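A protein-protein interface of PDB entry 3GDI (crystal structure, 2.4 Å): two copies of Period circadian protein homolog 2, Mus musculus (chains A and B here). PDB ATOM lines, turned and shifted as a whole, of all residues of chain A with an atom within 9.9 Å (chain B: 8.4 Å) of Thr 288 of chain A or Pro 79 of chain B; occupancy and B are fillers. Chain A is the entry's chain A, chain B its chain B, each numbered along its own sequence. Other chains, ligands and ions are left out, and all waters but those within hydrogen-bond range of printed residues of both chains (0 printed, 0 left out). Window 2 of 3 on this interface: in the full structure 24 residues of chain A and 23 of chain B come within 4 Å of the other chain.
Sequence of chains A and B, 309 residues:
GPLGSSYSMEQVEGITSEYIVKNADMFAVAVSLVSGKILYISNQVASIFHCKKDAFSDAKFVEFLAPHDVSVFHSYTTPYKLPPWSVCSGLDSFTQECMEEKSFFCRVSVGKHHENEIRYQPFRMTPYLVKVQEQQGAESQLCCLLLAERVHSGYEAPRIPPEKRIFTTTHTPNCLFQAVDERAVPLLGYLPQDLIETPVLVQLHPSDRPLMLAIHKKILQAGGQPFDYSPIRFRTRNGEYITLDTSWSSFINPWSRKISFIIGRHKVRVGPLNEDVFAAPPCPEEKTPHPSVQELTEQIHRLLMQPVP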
ATOM      1  N   LEU A 176     -12.763  -2.273  32.151  1.00  0.00           N
ATOM      2  CA  LEU A 176     -12.986  -3.709  32.262  1.00  0.00           C
ATOM      3  C   LEU A 176     -11.943  -4.189  33.277  1.00  0.00           C
ATOM      4  O   LEU A 176     -10.781  -3.778  33.211  1.00  0.00           O
ATOM      5  CB  LEU A 176     -12.733  -4.404  30.927  1.00  0.00           C
ATOM      6  CG  LEU A 176     -13.834  -4.457  29.875  1.00  0.00           C
ATOM      7  CD1 LEU A 176     -14.801  -3.301  30.065  1.00  0.00           C
ATOM      8  CD2 LEU A 176     -13.183  -4.452  28.487  1.00  0.00           C
ATOM      9  N   GLU A 197     -12.095  -8.933  32.495  1.00  0.00           N
ATOM     10  CA  GLU A 197     -12.613  -8.509  31.192  1.00  0.00           C
ATOM     11  C   GLU A 197     -14.094  -8.132  31.168  1.00  0.00           C
ATOM     12  O   GLU A 197     -14.691  -8.029  30.088  1.00  0.00           O
ATOM     13  CB  GLU A 197     -12.372  -9.590  30.132  1.00  0.00           C
ATOM     14  CG  GLU A 197     -10.917  -9.997  29.938  1.00  0.00           C
ATOM     15  CD  GLU A 197     -10.098  -8.950  29.216  1.00  0.00           C
ATOM     16  OE1 GLU A 197      -8.958  -9.270  28.821  1.00  0.00           O
ATOM     17  OE2 GLU A 197     -10.585  -7.814  29.045  1.00  0.00           O
ATOM     18  N   THR A 198     -14.695  -7.932  32.335  1.00  0.00           N
ATOM     19  CA  THR A 198     -16.100  -7.543  32.381  1.00  0.00           C
ATOM     20  C   THR A 198     -16.199  -6.108  32.901  1.00  0.00           C
ATOM     21  O   THR A 198     -15.295  -5.628  33.585  1.00  0.00           O
ATOM     22  CB  THR A 198     -16.915  -8.502  33.274  1.00  0.00           C
ATOM     23  OG1 THR A 198     -16.647  -8.236  34.654  1.00  0.00           O
ATOM     24  CG2 THR A 198     -16.536  -9.950  32.970  1.00  0.00           C
ATOM     25  N   PRO A 199     -17.304  -5.405  32.591  1.00  0.00           N
ATOM     26  CA  PRO A 199     -17.456  -4.022  33.053  1.00  0.00           C
ATOM     27  C   PRO A 199     -17.421  -3.876  34.558  1.00  0.00           C
ATOM     28  O   PRO A 199     -18.137  -4.562  35.274  1.00  0.00           O
ATOM     29  CB  PRO A 199     -18.815  -3.597  32.476  1.00  0.00           C
ATOM     30  CG  PRO A 199     -18.982  -4.481  31.264  1.00  0.00           C
ATOM     31  CD  PRO A 199     -18.481  -5.816  31.801  1.00  0.00           C
ATOM     32  N   VAL A 202     -20.782  -2.690  36.075  1.00  0.00           N
ATOM     33  CA  VAL A 202     -21.859  -3.661  36.186  1.00  0.00           C
ATOM     34  C   VAL A 202     -21.978  -4.192  37.615  1.00  0.00           C
ATOM     35  O   VAL A 202     -23.086  -4.367  38.130  1.00  0.00           O
ATOM     36  CB  VAL A 202     -21.655  -4.815  35.147  1.00  0.00           C
ATOM     37  CG1 VAL A 202     -22.147  -6.144  35.675  1.00  0.00           C
ATOM     38  CG2 VAL A 202     -22.417  -4.477  33.889  1.00  0.00           C
ATOM     39  N   ARG A 235     -21.687  -5.621  44.115  1.00  0.00           N
ATOM     40  CA  ARG A 235     -22.469  -6.848  44.087  1.00  0.00           C
ATOM     41  C   ARG A 235     -21.633  -8.120  44.185  1.00  0.00           C
ATOM     42  O   ARG A 235     -20.594  -8.250  43.537  1.00  0.00           O
ATOM     43  CB  ARG A 235     -23.321  -6.905  42.823  1.00  0.00           C
ATOM     44  CG  ARG A 235     -24.222  -8.134  42.746  1.00  0.00           C
ATOM     45  CD  ARG A 235     -25.394  -7.905  41.796  1.00  0.00           C
ATOM     46  NE  ARG A 235     -24.949  -7.386  40.509  1.00  0.00           N
ATOM     47  CZ  ARG A 235     -24.231  -8.081  39.633  1.00  0.00           C
ATOM     48  NH1 ARG A 235     -23.859  -7.527  38.487  1.00  0.00           N
ATOM     49  NH2 ARG A 235     -23.900  -9.338  39.900  1.00  0.00           N
ATOM     50  N   PRO A 284     -32.245 -14.234  37.178  1.00  0.00           N
ATOM     51  CA  PRO A 284     -31.892 -14.792  35.866  1.00  0.00           C
ATOM     52  C   PRO A 284     -30.533 -14.334  35.354  1.00  0.00           C
ATOM     53  O   PRO A 284     -30.450 -13.544  34.412  1.00  0.00           O
ATOM     54  CB  PRO A 284     -33.031 -14.313  34.970  1.00  0.00           C
ATOM     55  CG  PRO A 284     -34.193 -14.287  35.904  1.00  0.00           C
ATOM     56  CD  PRO A 284     -33.593 -13.637  37.136  1.00  0.00           C
ATOM     57  N   GLU A 285     -29.474 -14.847  35.976  1.00  0.00           N
ATOM     58  CA  GLU A 285     -28.103 -14.501  35.616  1.00  0.00           C
ATOM     59  C   GLU A 285     -27.967 -13.021  35.279  1.00  0.00           C
ATOM     60  O   GLU A 285     -28.823 -12.207  35.638  1.00  0.00           O
ATOM     61  CB  GLU A 285     -27.628 -15.338  34.423  1.00  0.00           C
ATOM     62  CG  GLU A 285     -27.526 -16.829  34.700  1.00  0.00           C
ATOM     63  CD  GLU A 285     -26.680 -17.555  33.668  1.00  0.00           C
ATOM     64  OE1 GLU A 285     -26.973 -17.429  32.459  1.00  0.00           O
ATOM     65  OE2 GLU A 285     -25.721 -18.253  34.065  1.00  0.00           O
ATOM     66  N   GLU A 286     -26.882 -12.679  34.596  1.00  0.00           N
ATOM     67  CA  GLU A 286     -26.644 -11.301  34.201  1.00  0.00           C
ATOM     68  C   GLU A 286     -27.388 -11.010  32.910  1.00  0.00           C
ATOM     69  O   GLU A 286     -28.405 -11.641  32.619  1.00  0.00           O
ATOM     70  CB  GLU A 286     -25.149 -11.052  34.016  1.00  0.00           C
ATOM     71  CG  GLU A 286     -24.391 -11.004  35.327  1.00  0.00           C
ATOM     72  CD  GLU A 286     -25.028 -10.043  36.315  1.00  0.00           C
ATOM     73  OE1 GLU A 286     -25.221  -8.860  35.958  1.00  0.00           O
ATOM     74  OE2 GLU A 286     -25.337 -10.471  37.448  1.00  0.00           O
ATOM     75  N   LYS A 287     -26.887 -10.055  32.136  1.00  0.00           N
ATOM     76  CA  LYS A 287     -27.535  -9.703  30.883  1.00  0.00           C
ATOM     77  C   LYS A 287     -26.531  -9.269  29.831  1.00  0.00           C
ATOM     78  O   LYS A 287     -25.480  -9.890  29.660  1.00  0.00           O
ATOM     79  CB  LYS A 287     -28.558  -8.587  31.117  1.00  0.00           C
ATOM     80  CG  LYS A 287     -29.756  -9.009  31.955  1.00  0.00           C
ATOM     81  CD  LYS A 287     -30.556 -10.102  31.258  1.00  0.00           C
ATOM     82  CE  LYS A 287     -31.659 -10.645  32.153  1.00  0.00           C
ATOM     83  NZ  LYS A 287     -32.604  -9.580  32.591  1.00  0.00           N
ATOM     84  N   THR A 288     -26.870  -8.196  29.129  1.00  0.00           N
ATOM     85  CA  THR A 288     -26.031  -7.646  28.075  1.00  0.00           C
ATOM     86  C   THR A 288     -26.369  -6.178  27.835  1.00  0.00           C
ATOM     87  O   THR A 288     -25.474  -5.355  27.639  1.00  0.00           O
ATOM     88  CB  THR A 288     -26.221  -8.420  26.754  1.00  0.00           C
ATOM     89  OG1 THR A 288     -25.748  -9.764  26.912  1.00  0.00           O
ATOM     90  CG2 THR A 288     -25.461  -7.745  25.622  1.00  0.00           C
ATOM     91  N   PRO A 289     -27.670  -5.832  27.845  1.00  0.00           N
ATOM     92  CA  PRO A 289     -28.109  -4.450  27.626  1.00  0.00           C
ATOM     93  C   PRO A 289     -27.228  -3.400  28.301  1.00  0.00           C
ATOM     94  O   PRO A 289     -26.383  -2.785  27.652  1.00  0.00           O
ATOM     95  CB  PRO A 289     -29.532  -4.464  28.162  1.00  0.00           C
ATOM     96  CG  PRO A 289     -30.008  -5.808  27.703  1.00  0.00           C
ATOM     97  CD  PRO A 289     -28.836  -6.715  28.050  1.00  0.00           C
ATOM     98  N   HIS A 290     -27.427  -3.190  29.597  1.00  0.00           N
ATOM     99  CA  HIS A 290     -26.623  -2.214  30.321  1.00  0.00           C
ATOM    100  C   HIS A 290     -26.752  -0.857  29.624  1.00  0.00           C
ATOM    101  O   HIS A 290     -25.753  -0.235  29.257  1.00  0.00           O
ATOM    102  CB  HIS A 290     -25.157  -2.655  30.311  1.00  0.00           C
ATOM    103  CG  HIS A 290     -24.957  -4.111  30.604  1.00  0.00           C
ATOM    104  ND1 HIS A 290     -23.783  -4.773  30.311  1.00  0.00           N
ATOM    105  CD2 HIS A 290     -25.774  -5.030  31.174  1.00  0.00           C
ATOM    106  CE1 HIS A 290     -23.885  -6.035  30.687  1.00  0.00           C
ATOM    107  NE2 HIS A 290     -25.083  -6.217  31.214  1.00  0.00           N
ATOM    108  N   PRO A 291     -27.990  -0.379  29.438  1.00  0.00           N
ATOM    109  CA  PRO A 291     -28.254   0.905  28.780  1.00  0.00           C
ATOM    110  C   PRO A 291     -27.315   2.021  29.225  1.00  0.00           C
ATOM    111  O   PRO A 291     -26.510   2.533  28.447  1.00  0.00           O
ATOM    112  CB  PRO A 291     -29.697   1.198  29.174  1.00  0.00           C
ATOM    113  CG  PRO A 291     -30.295  -0.173  29.281  1.00  0.00           C
ATOM    114  CD  PRO A 291     -29.227  -0.936  30.016  1.00  0.00           C
ATOM    115  N   SER A 292     -27.438   2.383  30.494  1.00  0.00           N
ATOM    116  CA  SER A 292     -26.644   3.445  31.084  1.00  0.00           C
ATOM    117  C   SER A 292     -25.184   3.075  31.324  1.00  0.00           C
ATOM    118  O   SER A 292     -24.312   3.943  31.285  1.00  0.00           O
ATOM    119  CB  SER A 292     -27.288   3.879  32.398  1.00  0.00           C
ATOM    120  OG  SER A 292     -28.653   4.185  32.194  1.00  0.00           O
ATOM    121  N   VAL A 293     -24.911   1.798  31.577  1.00  0.00           N
ATOM    122  CA  VAL A 293     -23.538   1.371  31.821  1.00  0.00           C
ATOM    123  C   VAL A 293     -22.646   1.655  30.623  1.00  0.00           C
ATOM    124  O   VAL A 293     -21.552   2.185  30.780  1.00  0.00           O
ATOM    125  CB  VAL A 293     -23.460  -0.126  32.166  1.00  0.00           C
ATOM    126  CG1 VAL A 293     -22.012  -0.588  32.199  1.00  0.00           C
ATOM    127  CG2 VAL A 293     -24.094  -0.363  33.517  1.00  0.00           C
ATOM    128  N   GLN A 294     -23.111   1.310  29.429  1.00  0.00           N
ATOM    129  CA  GLN A 294     -22.330   1.554  28.220  1.00  0.00           C
ATOM    130  C   GLN A 294     -22.002   3.041  28.132  1.00  0.00           C
ATOM    131  O   GLN A 294     -20.854   3.430  27.937  1.00  0.00           O
ATOM    132  CB  GLN A 294     -23.123   1.139  26.981  1.00  0.00           C
ATOM    133  CG  GLN A 294     -23.564  -0.317  26.971  1.00  0.00           C
ATOM    134  CD  GLN A 294     -24.461  -0.640  25.785  1.00  0.00           C
ATOM    135  OE1 GLN A 294     -24.921  -1.772  25.625  1.00  0.00           O
ATOM    136  NE2 GLN A 294     -24.712   0.360  24.945  1.00  0.00           N
ATOM    137  N   GLU A 295     -23.033   3.861  28.286  1.00  0.00           N
ATOM    138  CA  GLU A 295     -22.907   5.311  28.230  1.00  0.00           C
ATOM    139  C   GLU A 295     -21.871   5.860  29.203  1.00  0.00           C
ATOM    140  O   GLU A 295     -20.974   6.615  28.818  1.00  0.00           O
ATOM    141  CB  GLU A 295     -24.262   5.959  28.540  1.00  0.00           C
ATOM    142  CG  GLU A 295     -24.208   7.479  28.697  1.00  0.00           C
ATOM    143  CD  GLU A 295     -25.378   8.037  29.506  1.00  0.00           C
ATOM    144  OE1 GLU A 295     -25.435   9.276  29.693  1.00  0.00           O
ATOM    145  OE2 GLU A 295     -26.231   7.240  29.958  1.00  0.00           O
ATOM    146  N   THR A 297     -19.601   4.214  30.788  1.00  0.00           N
ATOM    147  CA  THR A 297     -18.320   3.587  30.540  1.00  0.00           C
ATOM    148  C   THR A 297     -17.516   4.371  29.509  1.00  0.00           C
ATOM    149  O   THR A 297     -16.417   4.830  29.798  1.00  0.00           O
ATOM    150  CB  THR A 297     -18.516   2.123  30.067  1.00  0.00           C
ATOM    151  OG1 THR A 297     -18.932   1.316  31.175  1.00  0.00           O
ATOM    152  CG2 THR A 297     -17.234   1.558  29.490  1.00  0.00           C
ATOM    153  N   LEU B  33     -24.231 -10.332  15.587  1.00  0.00           N
ATOM    154  CA  LEU B  33     -23.795 -10.790  16.897  1.00  0.00           C
ATOM    155  C   LEU B  33     -24.604 -12.005  17.322  1.00  0.00           C
ATOM    156  O   LEU B  33     -24.649 -12.355  18.498  1.00  0.00           O
ATOM    157  CB  LEU B  33     -23.933  -9.674  17.936  1.00  0.00           C
ATOM    158  CG  LEU B  33     -22.927  -8.522  17.832  1.00  0.00           C
ATOM    159  CD1 LEU B  33     -23.187  -7.514  18.939  1.00  0.00           C
ATOM    160  CD2 LEU B  33     -21.506  -9.067  17.933  1.00  0.00           C
ATOM    161  N   VAL B  34     -25.249 -12.644  16.351  1.00  0.00           N
ATOM    162  CA  VAL B  34     -26.044 -13.836  16.610  1.00  0.00           C
ATOM    163  C   VAL B  34     -25.796 -14.879  15.529  1.00  0.00           C
ATOM    164  O   VAL B  34     -26.072 -16.059  15.726  1.00  0.00           O
ATOM    165  CB  VAL B  34     -27.553 -13.516  16.652  1.00  0.00           C
ATOM    166  CG1 VAL B  34     -27.842 -12.506  17.747  1.00  0.00           C
ATOM    167  CG2 VAL B  34     -28.009 -12.984  15.311  1.00  0.00           C
ATOM    168  N   HIS B  74     -13.763 -13.131  18.957  1.00  0.00           N
ATOM    169  CA  HIS B  74     -14.950 -13.265  19.803  1.00  0.00           C
ATOM    170  C   HIS B  74     -14.829 -12.415  21.068  1.00  0.00           C
ATOM    171  O   HIS B  74     -15.756 -11.695  21.448  1.00  0.00           O
ATOM    172  CB  HIS B  74     -15.171 -14.730  20.216  1.00  0.00           C
ATOM    173  CG  HIS B  74     -15.586 -15.623  19.092  1.00  0.00           C
ATOM    174  ND1 HIS B  74     -16.576 -15.278  18.194  1.00  0.00           N
ATOM    175  CD2 HIS B  74     -15.144 -16.846  18.715  1.00  0.00           C
ATOM    176  CE1 HIS B  74     -16.723 -16.248  17.309  1.00  0.00           C
ATOM    177  NE2 HIS B  74     -15.867 -17.212  17.602  1.00  0.00           N
ATOM    178  N   SER B  75     -13.677 -12.506  21.719  1.00  0.00           N
ATOM    179  CA  SER B  75     -13.448 -11.756  22.937  1.00  0.00           C
ATOM    180  C   SER B  75     -13.594 -10.255  22.749  1.00  0.00           C
ATOM    181  O   SER B  75     -14.226  -9.584  23.563  1.00  0.00           O
ATOM    182  CB  SER B  75     -12.059 -12.053  23.483  1.00  0.00           C
ATOM    183  OG  SER B  75     -11.774 -11.181  24.561  1.00  0.00           O
ATOM    184  N   TYR B  76     -13.010  -9.721  21.684  1.00  0.00           N
ATOM    185  CA  TYR B  76     -13.085  -8.286  21.446  1.00  0.00           C
ATOM    186  C   TYR B  76     -14.419  -7.827  20.893  1.00  0.00           C
ATOM    187  O   TYR B  76     -14.667  -6.637  20.770  1.00  0.00           O
ATOM    188  CB  TYR B  76     -11.945  -7.849  20.523  1.00  0.00           C
ATOM    189  CG  TYR B  76     -10.619  -7.746  21.242  1.00  0.00           C
ATOM    190  CD1 TYR B  76     -10.214  -6.551  21.842  1.00  0.00           C
ATOM    191  CD2 TYR B  76      -9.789  -8.862  21.371  1.00  0.00           C
ATOM    192  CE1 TYR B  76      -9.016  -6.468  22.556  1.00  0.00           C
ATOM    193  CE2 TYR B  76      -8.590  -8.792  22.086  1.00  0.00           C
ATOM    194  CZ  TYR B  76      -8.212  -7.596  22.674  1.00  0.00           C
ATOM    195  OH  TYR B  76      -7.036  -7.538  23.378  1.00  0.00           O
ATOM    196  N   THR B  77     -15.290  -8.768  20.558  1.00  0.00           N
ATOM    197  CA  THR B  77     -16.598  -8.392  20.036  1.00  0.00           C
ATOM    198  C   THR B  77     -17.753  -8.825  20.928  1.00  0.00           C
ATOM    199  O   THR B  77     -18.897  -8.731  20.509  1.00  0.00           O
ATOM    200  CB  THR B  77     -16.852  -8.957  18.628  1.00  0.00           C
ATOM    201  OG1 THR B  77     -16.751 -10.382  18.664  1.00  0.00           O
ATOM    202  CG2 THR B  77     -15.852  -8.407  17.639  1.00  0.00           C
ATOM    203  N   THR B  78     -17.478  -9.301  22.144  1.00  0.00           N
ATOM    204  CA  THR B  78     -18.591  -9.680  23.018  1.00  0.00           C
ATOM    205  C   THR B  78     -19.316  -8.357  23.287  1.00  0.00           C
ATOM    206  O   THR B  78     -18.686  -7.336  23.566  1.00  0.00           O
ATOM    207  CB  THR B  78     -18.134 -10.314  24.376  1.00  0.00           C
ATOM    208  OG1 THR B  78     -17.717  -9.284  25.278  1.00  0.00           O
ATOM    209  CG2 THR B  78     -16.989 -11.289  24.168  1.00  0.00           C
ATOM    210  N   PRO B  79     -20.652  -8.358  23.204  1.00  0.00           N
ATOM    211  CA  PRO B  79     -21.457  -7.149  23.427  1.00  0.00           C
ATOM    212  C   PRO B  79     -21.052  -6.180  24.547  1.00  0.00           C
ATOM    213  O   PRO B  79     -21.017  -4.972  24.325  1.00  0.00           O
ATOM    214  CB  PRO B  79     -22.863  -7.713  23.626  1.00  0.00           C
ATOM    215  CG  PRO B  79     -22.858  -8.902  22.696  1.00  0.00           C
ATOM    216  CD  PRO B  79     -21.516  -9.536  23.004  1.00  0.00           C
ATOM    217  N   TYR B  80     -20.744  -6.697  25.737  1.00  0.00           N
ATOM    218  CA  TYR B  80     -20.394  -5.828  26.855  1.00  0.00           C
ATOM    219  C   TYR B  80     -19.002  -5.212  26.815  1.00  0.00           C
ATOM    220  O   TYR B  80     -18.455  -4.827  27.848  1.00  0.00           O
ATOM    221  CB  TYR B  80     -20.616  -6.550  28.196  1.00  0.00           C
ATOM    222  CG  TYR B  80     -19.704  -7.729  28.493  1.00  0.00           C
ATOM    223  CD1 TYR B  80     -20.233  -9.006  28.674  1.00  0.00           C
ATOM    224  CD2 TYR B  80     -18.319  -7.564  28.634  1.00  0.00           C
ATOM    225  CE1 TYR B  80     -19.416 -10.095  28.989  1.00  0.00           C
ATOM    226  CE2 TYR B  80     -17.486  -8.652  28.950  1.00  0.00           C
ATOM    227  CZ  TYR B  80     -18.047  -9.914  29.124  1.00  0.00           C
ATOM    228  OH  TYR B  80     -17.256 -11.005  29.419  1.00  0.00           O
ATOM    229  N   LYS B  81     -18.437  -5.107  25.616  1.00  0.00           N
ATOM    230  CA  LYS B  81     -17.114  -4.506  25.444  1.00  0.00           C
ATOM    231  C   LYS B  81     -17.170  -3.489  24.313  1.00  0.00           C
ATOM    232  O   LYS B  81     -16.448  -2.492  24.325  1.00  0.00           O
ATOM    233  CB  LYS B  81     -16.069  -5.571  25.106  1.00  0.00           C
ATOM    234  CG  LYS B  81     -15.907  -6.653  26.151  1.00  0.00           C
ATOM    235  CD  LYS B  81     -14.773  -7.586  25.778  1.00  0.00           C
ATOM    236  CE  LYS B  81     -14.581  -8.678  26.817  1.00  0.00           C
ATOM    237  NZ  LYS B  81     -13.470  -9.611  26.453  1.00  0.00           N
ATOM    238  N   LEU B  82     -18.040  -3.751  23.342  1.00  0.00           N
ATOM    239  CA  LEU B  82     -18.205  -2.890  22.176  1.00  0.00           C
ATOM    240  C   LEU B  82     -18.788  -1.521  22.508  1.00  0.00           C
ATOM    241  O   LEU B  82     -19.865  -1.414  23.098  1.00  0.00           O
ATOM    242  CB  LEU B  82     -19.102  -3.569  21.139  1.00  0.00           C
ATOM    243  CG  LEU B  82     -18.699  -4.960  20.650  1.00  0.00           C
ATOM    244  CD1 LEU B  82     -19.700  -5.418  19.604  1.00  0.00           C
ATOM    245  CD2 LEU B  82     -17.288  -4.933  20.076  1.00  0.00           C
ATOM    246  N   PRO B  83     -18.073  -0.449  22.138  1.00  0.00           N
ATOM    247  CA  PRO B  83     -18.535   0.918  22.396  1.00  0.00           C
ATOM    248  C   PRO B  83     -19.697   1.263  21.470  1.00  0.00           C
ATOM    249  O   PRO B  83     -19.536   1.276  20.248  1.00  0.00           O
ATOM    250  CB  PRO B  83     -17.300   1.768  22.094  1.00  0.00           C
ATOM    251  CG  PRO B  83     -16.150   0.824  22.351  1.00  0.00           C
ATOM    252  CD  PRO B  83     -16.656  -0.452  21.729  1.00  0.00           C
ATOM    253  N   TYR B 128     -17.135  -1.776  16.591  1.00  0.00           N
ATOM    254  CA  TYR B 128     -18.170  -0.817  16.979  1.00  0.00           C
ATOM    255  C   TYR B 128     -19.532  -1.517  17.036  1.00  0.00           C
ATOM    256  O   TYR B 128     -19.904  -2.243  16.110  1.00  0.00           O
ATOM    257  CB  TYR B 128     -18.228   0.325  15.962  1.00  0.00           C
ATOM    258  CG  TYR B 128     -17.014   1.236  15.973  1.00  0.00           C
ATOM    259  CD1 TYR B 128     -16.457   1.702  14.778  1.00  0.00           C
ATOM    260  CD2 TYR B 128     -16.440   1.660  17.175  1.00  0.00           C
ATOM    261  CE1 TYR B 128     -15.362   2.564  14.780  1.00  0.00           C
ATOM    262  CE2 TYR B 128     -15.347   2.522  17.187  1.00  0.00           C
ATOM    263  CZ  TYR B 128     -14.815   2.971  15.987  1.00  0.00           C
ATOM    264  OH  TYR B 128     -13.745   3.837  15.990  1.00  0.00           O
ATOM    265  N   LEU B 129     -20.277  -1.291  18.113  1.00  0.00           N
ATOM    266  CA  LEU B 129     -21.585  -1.922  18.275  1.00  0.00           C
ATOM    267  C   LEU B 129     -22.722  -1.156  17.613  1.00  0.00           C
ATOM    268  O   LEU B 129     -23.278  -0.232  18.210  1.00  0.00           O
ATOM    269  CB  LEU B 129     -21.926  -2.080  19.754  1.00  0.00           C
ATOM    270  CG  LEU B 129     -23.242  -2.832  19.960  1.00  0.00           C
ATOM    271  CD1 LEU B 129     -22.944  -4.320  19.994  1.00  0.00           C
ATOM    272  CD2 LEU B 129     -23.918  -2.396  21.250  1.00  0.00           C
ATOM    273  N   LEU B 142     -28.807  -6.432  15.660  1.00  0.00           N
ATOM    274  CA  LEU B 142     -27.712  -5.897  16.466  1.00  0.00           C
ATOM    275  C   LEU B 142     -26.394  -6.434  15.914  1.00  0.00           C
ATOM    276  O   LEU B 142     -26.071  -7.610  16.077  1.00  0.00           O
ATOM    277  CB  LEU B 142     -27.883  -6.313  17.930  1.00  0.00           C
ATOM    278  CG  LEU B 142     -27.266  -5.390  18.984  1.00  0.00           C
ATOM    279  CD1 LEU B 142     -25.765  -5.333  18.791  1.00  0.00           C
ATOM    280  CD2 LEU B 142     -27.876  -3.994  18.878  1.00  0.00           C
ATOM    281  N   CYS B 143     -25.630  -5.561  15.269  1.00  0.00           N
ATOM    282  CA  CYS B 143     -24.373  -5.971  14.660  1.00  0.00           C
ATOM    283  C   CYS B 143     -23.121  -5.321  15.218  1.00  0.00           C
ATOM    284  O   CYS B 143     -23.176  -4.394  16.026  1.00  0.00           O
ATOM    285  CB  CYS B 143     -24.427  -5.704  13.155  1.00  0.00           C
ATOM    286  SG  CYS B 143     -25.846  -6.452  12.334  1.00  0.00           S
ATOM    287  N   CYS B 144     -21.987  -5.834  14.757  1.00  0.00           N
ATOM    288  CA  CYS B 144     -20.675  -5.337  15.139  1.00  0.00           C
ATOM    289  C   CYS B 144     -20.019  -4.857  13.853  1.00  0.00           C
ATOM    290  O   CYS B 144     -19.704  -5.667  12.982  1.00  0.00           O
ATOM    291  CB  CYS B 144     -19.840  -6.460  15.752  1.00  0.00           C
ATOM    292  SG  CYS B 144     -18.165  -5.973  16.207  1.00  0.00           S
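A ring nitrogen (ND1) of His 290 of chain A sits at hydrogen-bond distance from the backbone carbonyl oxygen of Thr 288 of chain A (3.2 Å). The side-chain hydroxyl (OG) of Ser 75 of chain B sits at hydrogen-bond distance from the side-chain amino group (NZ) of Lys 81 of chain B, at 3.0 Å.
O of Glu 197 of chain A touches CE2 of Tyr 80 of chain B (3.1 Å). Glu 197 of chain A touches Lys 81 of chain B (O to CE, 3.3 Å). Tyr 80 of chain B touches Thr 198 of chain A (OH to CG2, 3.8 Å). Tyr 80 of chain B touches Pro 199 of chain A. CB of Pro 79 of chain B touches CG2 of Thr 288 of chain A, at 3.3 Å.
Of the printed residues of chain B, Glu 197 of chain A touches Tyr 80 (3.1 Å) and Lys 81 (3.3 Å). Of the printed residues of chain B, Thr 198 of chain A touches Tyr 80 (3.8 Å). Of the printed residues of chain B, Thr 288 of chain A touches Pro 79 (3.3 Å). No residue of chain B comes within 4 Å of Pro 289 of chain A. Of chain A, only Thr 288 comes within 4 Å of Pro 79 of chain B. No residue of chain A comes within 4 Å of Leu 82 of chain B. The nearest residue of chain B that does not touch Thr 288 of chain A is Tyr 80 of chain B (4.8 Å). The nearest printed residue of chain B that does not touch Thr 198 of chain A is Lys 81 of chain B (5.6 Å).
Of the 19 printed residues of chain A, 4 touch a printed residue of chain B. Of the 17 printed residues of chain B, 3 touch a printed residue of chain A. Among the printed residues, 5 pairs touch across the chains.
No position is printed for both chains. Of the 5 pairs that touch across the chains among the printed residues, none has its exchanged pair printed and touching as well.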
